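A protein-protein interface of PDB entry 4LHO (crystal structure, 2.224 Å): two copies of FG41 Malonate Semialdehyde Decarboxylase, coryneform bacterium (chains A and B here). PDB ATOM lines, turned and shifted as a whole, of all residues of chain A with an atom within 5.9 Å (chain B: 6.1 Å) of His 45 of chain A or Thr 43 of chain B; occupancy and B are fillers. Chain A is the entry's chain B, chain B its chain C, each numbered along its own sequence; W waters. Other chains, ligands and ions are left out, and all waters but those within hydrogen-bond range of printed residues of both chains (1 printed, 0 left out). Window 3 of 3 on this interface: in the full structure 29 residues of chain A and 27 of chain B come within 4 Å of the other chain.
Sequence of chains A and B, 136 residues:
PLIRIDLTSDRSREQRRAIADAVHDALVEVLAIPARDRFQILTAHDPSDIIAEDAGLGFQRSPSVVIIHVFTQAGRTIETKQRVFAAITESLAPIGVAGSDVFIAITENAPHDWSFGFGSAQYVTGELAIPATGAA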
ATOM      1  N   ASP A   6     -16.144  -2.045  -7.495  1.00  0.00           N
ATOM      2  CA  ASP A   6     -14.961  -1.434  -8.103  1.00  0.00           C
ATOM      3  C   ASP A   6     -15.366  -0.625  -9.288  1.00  0.00           C
ATOM      4  O   ASP A   6     -15.975  -1.128 -10.234  1.00  0.00           O
ATOM      5  CB  ASP A   6     -13.941  -2.487  -8.505  1.00  0.00           C
ATOM      6  CG  ASP A   6     -13.246  -3.110  -7.293  1.00  0.00           C
ATOM      7  OD1 ASP A   6     -12.093  -2.722  -7.026  1.00  0.00           O
ATOM      8  OD2 ASP A   6     -13.856  -3.963  -6.590  1.00  0.00           O
ATOM      9  N   LEU A   7     -15.055   0.656  -9.220  1.00  0.00           N
ATOM     10  CA  LEU A   7     -15.435   1.562 -10.277  1.00  0.00           C
ATOM     11  C   LEU A   7     -14.287   2.510 -10.632  1.00  0.00           C
ATOM     12  O   LEU A   7     -13.144   2.292 -10.244  1.00  0.00           O
ATOM     13  CB  LEU A   7     -16.701   2.290  -9.860  1.00  0.00           C
ATOM     14  CG  LEU A   7     -16.761   2.765  -8.406  1.00  0.00           C
ATOM     15  CD1 LEU A   7     -15.834   3.952  -8.200  1.00  0.00           C
ATOM     16  CD2 LEU A   7     -18.169   3.116  -8.035  1.00  0.00           C
ATOM     17  N   THR A   8     -14.580   3.540 -11.399  1.00  0.00           N
ATOM     18  CA  THR A   8     -13.529   4.369 -11.953  1.00  0.00           C
ATOM     19  C   THR A   8     -13.551   5.785 -11.357  1.00  0.00           C
ATOM     20  O   THR A   8     -14.599   6.297 -10.958  1.00  0.00           O
ATOM     21  CB  THR A   8     -13.606   4.402 -13.493  1.00  0.00           C
ATOM     22  OG1 THR A   8     -14.889   4.893 -13.916  1.00  0.00           O
ATOM     23  CG2 THR A   8     -13.380   3.029 -14.043  1.00  0.00           C
ATOM     24  N   SER A   9     -12.370   6.393 -11.289  1.00  0.00           N
ATOM     25  CA  SER A   9     -12.164   7.640 -10.540  1.00  0.00           C
ATOM     26  C   SER A   9     -12.834   8.859 -11.177  1.00  0.00           C
ATOM     27  O   SER A   9     -13.017   9.874 -10.511  1.00  0.00           O
ATOM     28  CB  SER A   9     -10.669   7.912 -10.392  1.00  0.00           C
ATOM     29  OG  SER A   9     -10.070   7.968 -11.674  1.00  0.00           O
ATOM     30  N   ASP A  10     -13.195   8.767 -12.457  1.00  0.00           N
ATOM     31  CA  ASP A  10     -13.869   9.875 -13.125  1.00  0.00           C
ATOM     32  C   ASP A  10     -15.224  10.158 -12.493  1.00  0.00           C
ATOM     33  O   ASP A  10     -15.779  11.222 -12.694  1.00  0.00           O
ATOM     34  CB  ASP A  10     -14.039   9.603 -14.620  1.00  0.00           C
ATOM     35  CG  ASP A  10     -14.864   8.348 -14.897  1.00  0.00           C
ATOM     36  OD1 ASP A  10     -16.060   8.454 -15.232  1.00  0.00           O
ATOM     37  OD2 ASP A  10     -14.307   7.250 -14.768  1.00  0.00           O
ATOM     38  N   THR A  43     -13.919   0.819  -4.199  1.00  0.00           N
ATOM     39  CA  THR A  43     -12.579   1.126  -4.637  1.00  0.00           C
ATOM     40  C   THR A  43     -12.624   1.817  -5.997  1.00  0.00           C
ATOM     41  O   THR A  43     -13.126   1.256  -6.973  1.00  0.00           O
ATOM     42  CB  THR A  43     -11.764  -0.148  -4.776  1.00  0.00           C
ATOM     43  OG1 THR A  43     -11.913  -0.934  -3.598  1.00  0.00           O
ATOM     44  CG2 THR A  43     -10.313   0.170  -4.998  1.00  0.00           C
ATOM     45  N   ALA A  44     -12.092   3.029  -6.063  1.00  0.00           N
ATOM     46  CA  ALA A  44     -11.985   3.758  -7.328  1.00  0.00           C
ATOM     47  C   ALA A  44     -10.657   3.471  -8.023  1.00  0.00           C
ATOM     48  O   ALA A  44      -9.621   3.376  -7.393  1.00  0.00           O
ATOM     49  CB  ALA A  44     -12.154   5.239  -7.105  1.00  0.00           C
ATOM     50  N   HIS A  45     -10.709   3.305  -9.334  1.00  0.00           N
ATOM     51  CA  HIS A  45      -9.522   2.969 -10.101  1.00  0.00           C
ATOM     52  C   HIS A  45      -9.382   3.954 -11.227  1.00  0.00           C
ATOM     53  O   HIS A  45     -10.343   4.627 -11.611  1.00  0.00           O
ATOM     54  CB  HIS A  45      -9.635   1.598 -10.735  1.00  0.00           C
ATOM     55  CG  HIS A  45      -9.754   0.478  -9.763  1.00  0.00           C
ATOM     56  ND1 HIS A  45      -8.714  -0.382  -9.493  1.00  0.00           N
ATOM     57  CD2 HIS A  45     -10.808   0.036  -9.037  1.00  0.00           C
ATOM     58  CE1 HIS A  45      -9.118  -1.294  -8.627  1.00  0.00           C
ATOM     59  NE2 HIS A  45     -10.383  -1.058  -8.333  1.00  0.00           N
ATOM     60  N   ASP A  46      -8.177   4.047 -11.767  1.00  0.00           N
ATOM     61  CA  ASP A  46      -8.030   4.740 -13.029  1.00  0.00           C
ATOM     62  C   ASP A  46      -8.765   3.870 -14.041  1.00  0.00           C
ATOM     63  O   ASP A  46      -8.689   2.650 -13.970  1.00  0.00           O
ATOM     64  CB  ASP A  46      -6.562   4.921 -13.431  1.00  0.00           C
ATOM     65  CG  ASP A  46      -6.424   5.715 -14.737  1.00  0.00           C
ATOM     66  OD1 ASP A  46      -6.467   6.963 -14.657  1.00  0.00           O
ATOM     67  OD2 ASP A  46      -6.317   5.112 -15.840  1.00  0.00           O
ATOM     68  N   PRO A  47      -9.473   4.494 -14.986  1.00  0.00           N
ATOM     69  CA  PRO A  47     -10.251   3.752 -15.977  1.00  0.00           C
ATOM     70  C   PRO A  47      -9.471   2.619 -16.647  1.00  0.00           C
ATOM     71  O   PRO A  47     -10.035   1.559 -16.895  1.00  0.00           O
ATOM     72  CB  PRO A  47     -10.627   4.843 -16.987  1.00  0.00           C
ATOM     73  CG  PRO A  47     -10.748   6.058 -16.160  1.00  0.00           C
ATOM     74  CD  PRO A  47      -9.685   5.947 -15.106  1.00  0.00           C
ATOM     75  N   ASP A  49      -7.462   0.638 -15.431  1.00  0.00           N
ATOM     76  CA  ASP A  49      -7.246  -0.495 -14.533  1.00  0.00           C
ATOM     77  C   ASP A  49      -8.458  -1.409 -14.470  1.00  0.00           C
ATOM     78  O   ASP A  49      -8.369  -2.502 -13.917  1.00  0.00           O
ATOM     79  CB  ASP A  49      -6.883  -0.007 -13.127  1.00  0.00           C
ATOM     80  CG  ASP A  49      -5.491   0.605 -13.075  1.00  0.00           C
ATOM     81  OD1 ASP A  49      -4.553  -0.033 -13.581  1.00  0.00           O
ATOM     82  OD2 ASP A  49      -5.346   1.739 -12.566  1.00  0.00           O
ATOM     83  N   ILE A  50      -9.590  -0.971 -15.023  1.00  0.00           N
ATOM     84  CA  ILE A  50     -10.705  -1.881 -15.204  1.00  0.00           C
ATOM     85  C   ILE A  50     -10.936  -2.191 -16.671  1.00  0.00           C
ATOM     86  O   ILE A  50     -11.208  -1.321 -17.456  1.00  0.00           O
ATOM     87  CB  ILE A  50     -11.982  -1.357 -14.613  1.00  0.00           C
ATOM     88  CG1 ILE A  50     -11.807  -1.131 -13.119  1.00  0.00           C
ATOM     89  CG2 ILE A  50     -13.079  -2.393 -14.836  1.00  0.00           C
ATOM     90  CD1 ILE A  50     -13.014  -0.640 -12.453  1.00  0.00           C
ATOM     91  N   ARG B   4      -8.893 -10.639 -10.593  1.00  0.00           N
ATOM     92  CA  ARG B   4      -8.328  -9.539  -9.802  1.00  0.00           C
ATOM     93  C   ARG B   4      -6.801  -9.702  -9.834  1.00  0.00           C
ATOM     94  O   ARG B   4      -6.236 -10.756  -9.433  1.00  0.00           O
ATOM     95  CB  ARG B   4      -8.836  -9.541  -8.352  1.00  0.00           C
ATOM     96  CG  ARG B   4     -10.273  -9.201  -8.211  1.00  0.00           C
ATOM     97  CD  ARG B   4     -10.725  -9.036  -6.761  1.00  0.00           C
ATOM     98  NE  ARG B   4     -12.185  -8.945  -6.779  1.00  0.00           N
ATOM     99  CZ  ARG B   4     -12.889  -7.818  -6.744  1.00  0.00           C
ATOM    100  NH1 ARG B   4     -12.294  -6.621  -6.598  1.00  0.00           N
ATOM    101  NH2 ARG B   4     -14.203  -7.896  -6.825  1.00  0.00           N
ATOM    102  N   ILE B   5      -6.156  -8.677 -10.384  1.00  0.00           N
ATOM    103  CA  ILE B   5      -4.711  -8.589 -10.422  1.00  0.00           C
ATOM    104  C   ILE B   5      -4.230  -7.509  -9.427  1.00  0.00           C
ATOM    105  O   ILE B   5      -4.516  -6.317  -9.578  1.00  0.00           O
ATOM    106  CB  ILE B   5      -4.225  -8.279 -11.842  1.00  0.00           C
ATOM    107  CG1 ILE B   5      -4.769  -9.331 -12.832  1.00  0.00           C
ATOM    108  CG2 ILE B   5      -2.738  -8.287 -11.868  1.00  0.00           C
ATOM    109  CD1 ILE B   5      -4.369  -9.130 -14.225  1.00  0.00           C
ATOM    110  N   ASP B   6      -3.521  -7.962  -8.400  1.00  0.00           N
ATOM    111  CA  ASP B   6      -2.971  -7.091  -7.376  1.00  0.00           C
ATOM    112  C   ASP B   6      -1.449  -7.115  -7.471  1.00  0.00           C
ATOM    113  O   ASP B   6      -0.811  -8.171  -7.333  1.00  0.00           O
ATOM    114  CB  ASP B   6      -3.474  -7.523  -6.004  1.00  0.00           C
ATOM    115  CG  ASP B   6      -4.957  -7.198  -5.797  1.00  0.00           C
ATOM    116  OD1 ASP B   6      -5.224  -6.128  -5.245  1.00  0.00           O
ATOM    117  OD2 ASP B   6      -5.849  -8.004  -6.177  1.00  0.00           O
ATOM    118  N   LEU B   7      -0.889  -5.951  -7.799  1.00  0.00           N
ATOM    119  CA  LEU B   7       0.523  -5.826  -8.053  1.00  0.00           C
ATOM    120  C   LEU B   7       0.988  -4.519  -7.435  1.00  0.00           C
ATOM    121  O   LEU B   7       0.247  -3.889  -6.692  1.00  0.00           O
ATOM    122  CB  LEU B   7       0.839  -5.926  -9.567  1.00  0.00           C
ATOM    123  CG  LEU B   7      -0.062  -5.088 -10.489  1.00  0.00           C
ATOM    124  CD1 LEU B   7       0.091  -3.616 -10.239  1.00  0.00           C
ATOM    125  CD2 LEU B   7       0.246  -5.378 -11.927  1.00  0.00           C
ATOM    126  N   THR B   8       2.225  -4.132  -7.736  1.00  0.00           N
ATOM    127  CA  THR B   8       2.876  -3.035  -7.045  1.00  0.00           C
ATOM    128  C   THR B   8       3.034  -1.856  -7.960  1.00  0.00           C
ATOM    129  O   THR B   8       3.278  -1.981  -9.177  1.00  0.00           O
ATOM    130  CB  THR B   8       4.304  -3.441  -6.446  1.00  0.00           C
ATOM    131  OG1 THR B   8       5.184  -3.863  -7.492  1.00  0.00           O
ATOM    132  CG2 THR B   8       4.178  -4.557  -5.455  1.00  0.00           C
ATOM    133  N   ILE B  41      -9.739  -6.476 -13.000  1.00  0.00           N
ATOM    134  CA  ILE B  41      -9.514  -5.337 -12.145  1.00  0.00           C
ATOM    135  C   ILE B  41      -8.037  -5.368 -11.712  1.00  0.00           C
ATOM    136  O   ILE B  41      -7.590  -6.271 -11.014  1.00  0.00           O
ATOM    137  CB  ILE B  41     -10.444  -5.393 -10.908  1.00  0.00           C
ATOM    138  CG1 ILE B  41     -11.905  -5.515 -11.371  1.00  0.00           C
ATOM    139  CG2 ILE B  41     -10.284  -4.156 -10.022  1.00  0.00           C
ATOM    140  CD1 ILE B  41     -12.855  -5.920 -10.274  1.00  0.00           C
ATOM    141  N   LEU B  42      -7.275  -4.389 -12.160  1.00  0.00           N
ATOM    142  CA  LEU B  42      -5.906  -4.239 -11.701  1.00  0.00           C
ATOM    143  C   LEU B  42      -5.854  -3.248 -10.556  1.00  0.00           C
ATOM    144  O   LEU B  42      -6.363  -2.147 -10.671  1.00  0.00           O
ATOM    145  CB  LEU B  42      -5.013  -3.755 -12.823  1.00  0.00           C
ATOM    146  CG  LEU B  42      -4.557  -4.885 -13.725  1.00  0.00           C
ATOM    147  CD1 LEU B  42      -5.525  -5.065 -14.894  1.00  0.00           C
ATOM    148  CD2 LEU B  42      -3.109  -4.660 -14.200  1.00  0.00           C
ATOM    149  N   THR B  43      -5.230  -3.645  -9.454  1.00  0.00           N
ATOM    150  CA  THR B  43      -5.076  -2.739  -8.346  1.00  0.00           C
ATOM    151  C   THR B  43      -3.591  -2.654  -7.977  1.00  0.00           C
ATOM    152  O   THR B  43      -2.981  -3.656  -7.593  1.00  0.00           O
ATOM    153  CB  THR B  43      -5.911  -3.182  -7.111  1.00  0.00           C
ATOM    154  OG1 THR B  43      -7.256  -3.501  -7.519  1.00  0.00           O
ATOM    155  CG2 THR B  43      -5.930  -2.043  -6.047  1.00  0.00           C
ATOM    156  N   ALA B  44      -3.045  -1.446  -8.080  1.00  0.00           N
ATOM    157  CA  ALA B  44      -1.669  -1.164  -7.682  1.00  0.00           C
ATOM    158  C   ALA B  44      -1.601  -0.793  -6.205  1.00  0.00           C
ATOM    159  O   ALA B  44      -2.447  -0.051  -5.690  1.00  0.00           O
ATOM    160  CB  ALA B  44      -1.084  -0.072  -8.544  1.00  0.00           C
ATOM    161  N   HIS B  45      -0.630  -1.367  -5.512  1.00  0.00           N
ATOM    162  CA  HIS B  45      -0.383  -1.074  -4.095  1.00  0.00           C
ATOM    163  C   HIS B  45       1.070  -0.649  -3.873  1.00  0.00           C
ATOM    164  O   HIS B  45       1.942  -0.985  -4.680  1.00  0.00           O
ATOM    165  CB  HIS B  45      -0.584  -2.338  -3.267  1.00  0.00           C
ATOM    166  CG  HIS B  45      -1.885  -3.013  -3.504  1.00  0.00           C
ATOM    167  ND1 HIS B  45      -2.966  -2.840  -2.676  1.00  0.00           N
ATOM    168  CD2 HIS B  45      -2.278  -3.879  -4.468  1.00  0.00           C
ATOM    169  CE1 HIS B  45      -3.974  -3.562  -3.119  1.00  0.00           C
ATOM    170  NE2 HIS B  45      -3.575  -4.204  -4.201  1.00  0.00           N
ATOM    171  N   ILE B  50       1.691  -5.494  -0.004  1.00  0.00           N
ATOM    172  CA  ILE B  50       1.523  -6.885  -0.419  1.00  0.00           C
ATOM    173  C   ILE B  50       2.582  -7.700   0.285  1.00  0.00           C
ATOM    174  O   ILE B  50       3.775  -7.443   0.144  1.00  0.00           O
ATOM    175  CB  ILE B  50       1.636  -7.109  -1.965  1.00  0.00           C
ATOM    176  CG1 ILE B  50       0.562  -6.326  -2.725  1.00  0.00           C
ATOM    177  CG2 ILE B  50       1.517  -8.583  -2.297  1.00  0.00           C
ATOM    178  CD1 ILE B  50       0.587  -6.561  -4.224  1.00  0.00           C
HETATM  179  O   HOH W   1     -15.685  -5.644  -7.317  1.00  0.00           O
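The guanidinium group of Arg 4 of chain B is in salt-bridge range of the side-chain carboxylate of Asp 6 of chain A, at 3.1 Å.
ND1 of His 45 of chain A lies within hydrogen-bond range of O of Leu 42 of chain B (3.2 Å).
The backbone carbonyl oxygen of Asp 49 of chain A lies within hydrogen-bond range of the backbone NH of Leu 42 of chain B (2.8 Å).
NE2 of His 45 of chain A sits at hydrogen-bond distance from OD1 of Asp 6 of chain A (2.7 Å).
N of His 45 of chain A is in hydrogen-bond range of O of Leu 7 of chain A, 2.8 Å away.
N of Ser 9 of chain A is in hydrogen-bond range of O of His 45 of chain A (2.7 Å).
The backbone carbonyl oxygen of Ile 5 of chain B sits at hydrogen-bond distance from the backbone NH of Thr 43 of chain B (2.8 Å).
The backbone NH (N) of Leu 7 of chain B lies within hydrogen-bond range of the backbone carbonyl oxygen (O) of Thr 43 of chain B, at 3.1 Å.
The backbone carbonyl oxygen (O) of Thr 43 of chain B sits close to a ring nitrogen (NE2) of His 45 of chain B, 3.5 Å away.
Among the printed residues, merely in contact across the chains: His 45 of chain A with Thr 43 of chain B, His 45 of chain A with Ile 41 of chain B, Asp 49 of chain A with Ile 41 of chain B and Asp 6 of chain A with Ile 41 of chain B.
Of the printed residues of chain B, His 45 of chain A touches Ile 41 (3.4 Å), Leu 42 (3.2 Å) and Thr 43 (3.1 Å).
Of chain A, only His 45 (3.1 Å) comes within 4 Å of Thr 43 of chain B.
Of the printed residues of chain A, Leu 42 of chain B touches His 45 (3.2 Å) and Asp 49 (2.8 Å).
Of the printed residues of chain B, Asp 49 of chain A touches Ile 41 (3.5 Å) and Leu 42 (2.8 Å).
Printed residues of chain A within 4 Å of Arg 4 of chain B: Asp 6.
Ile 50 of chain A touches none of the printed residues of chain B.
The nearest residue of chain A that does not touch Thr 43 of chain B is Asp 6 of chain A (4.9 Å).
The nearest printed residue of chain B that does not touch Asp 49 of chain A is Thr 43 of chain B (5.4 Å).
Along chain A the printed residues that touch a printed residue of chain B span positions 6 to 49.
Of the 11 printed residues of chain B, 4 touch a printed residue of chain A.
Printed residues of chain B that touch a printed residue of chain A: Arg 4, Ile 41, Leu 42 and Thr 43.
Hydrophobic or aromatic side chains of chain B that line the printed part of chain A: Ile 41 and Leu 42.
Among the printed residues, 7 pairs touch across the chains.
Among the printed residues, Asp or Glu carboxylates within 4 Å of a Lys or Arg side-chain nitrogen of the other chain: Asp 6 of chain A with Arg 4 of chain B (3.1 Å).
His 45 of chain A touches Thr 43 of chain B, but with the chains exchanged Thr 43 of chain A does not touch His 45 of chain B (7.6 Å).
Water W1 lies within hydrogen-bond range of the side-chain carboxylate (OD2) of Asp 6 of chain A and the guanidinium group (NH2) of Arg 4 of chain B.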
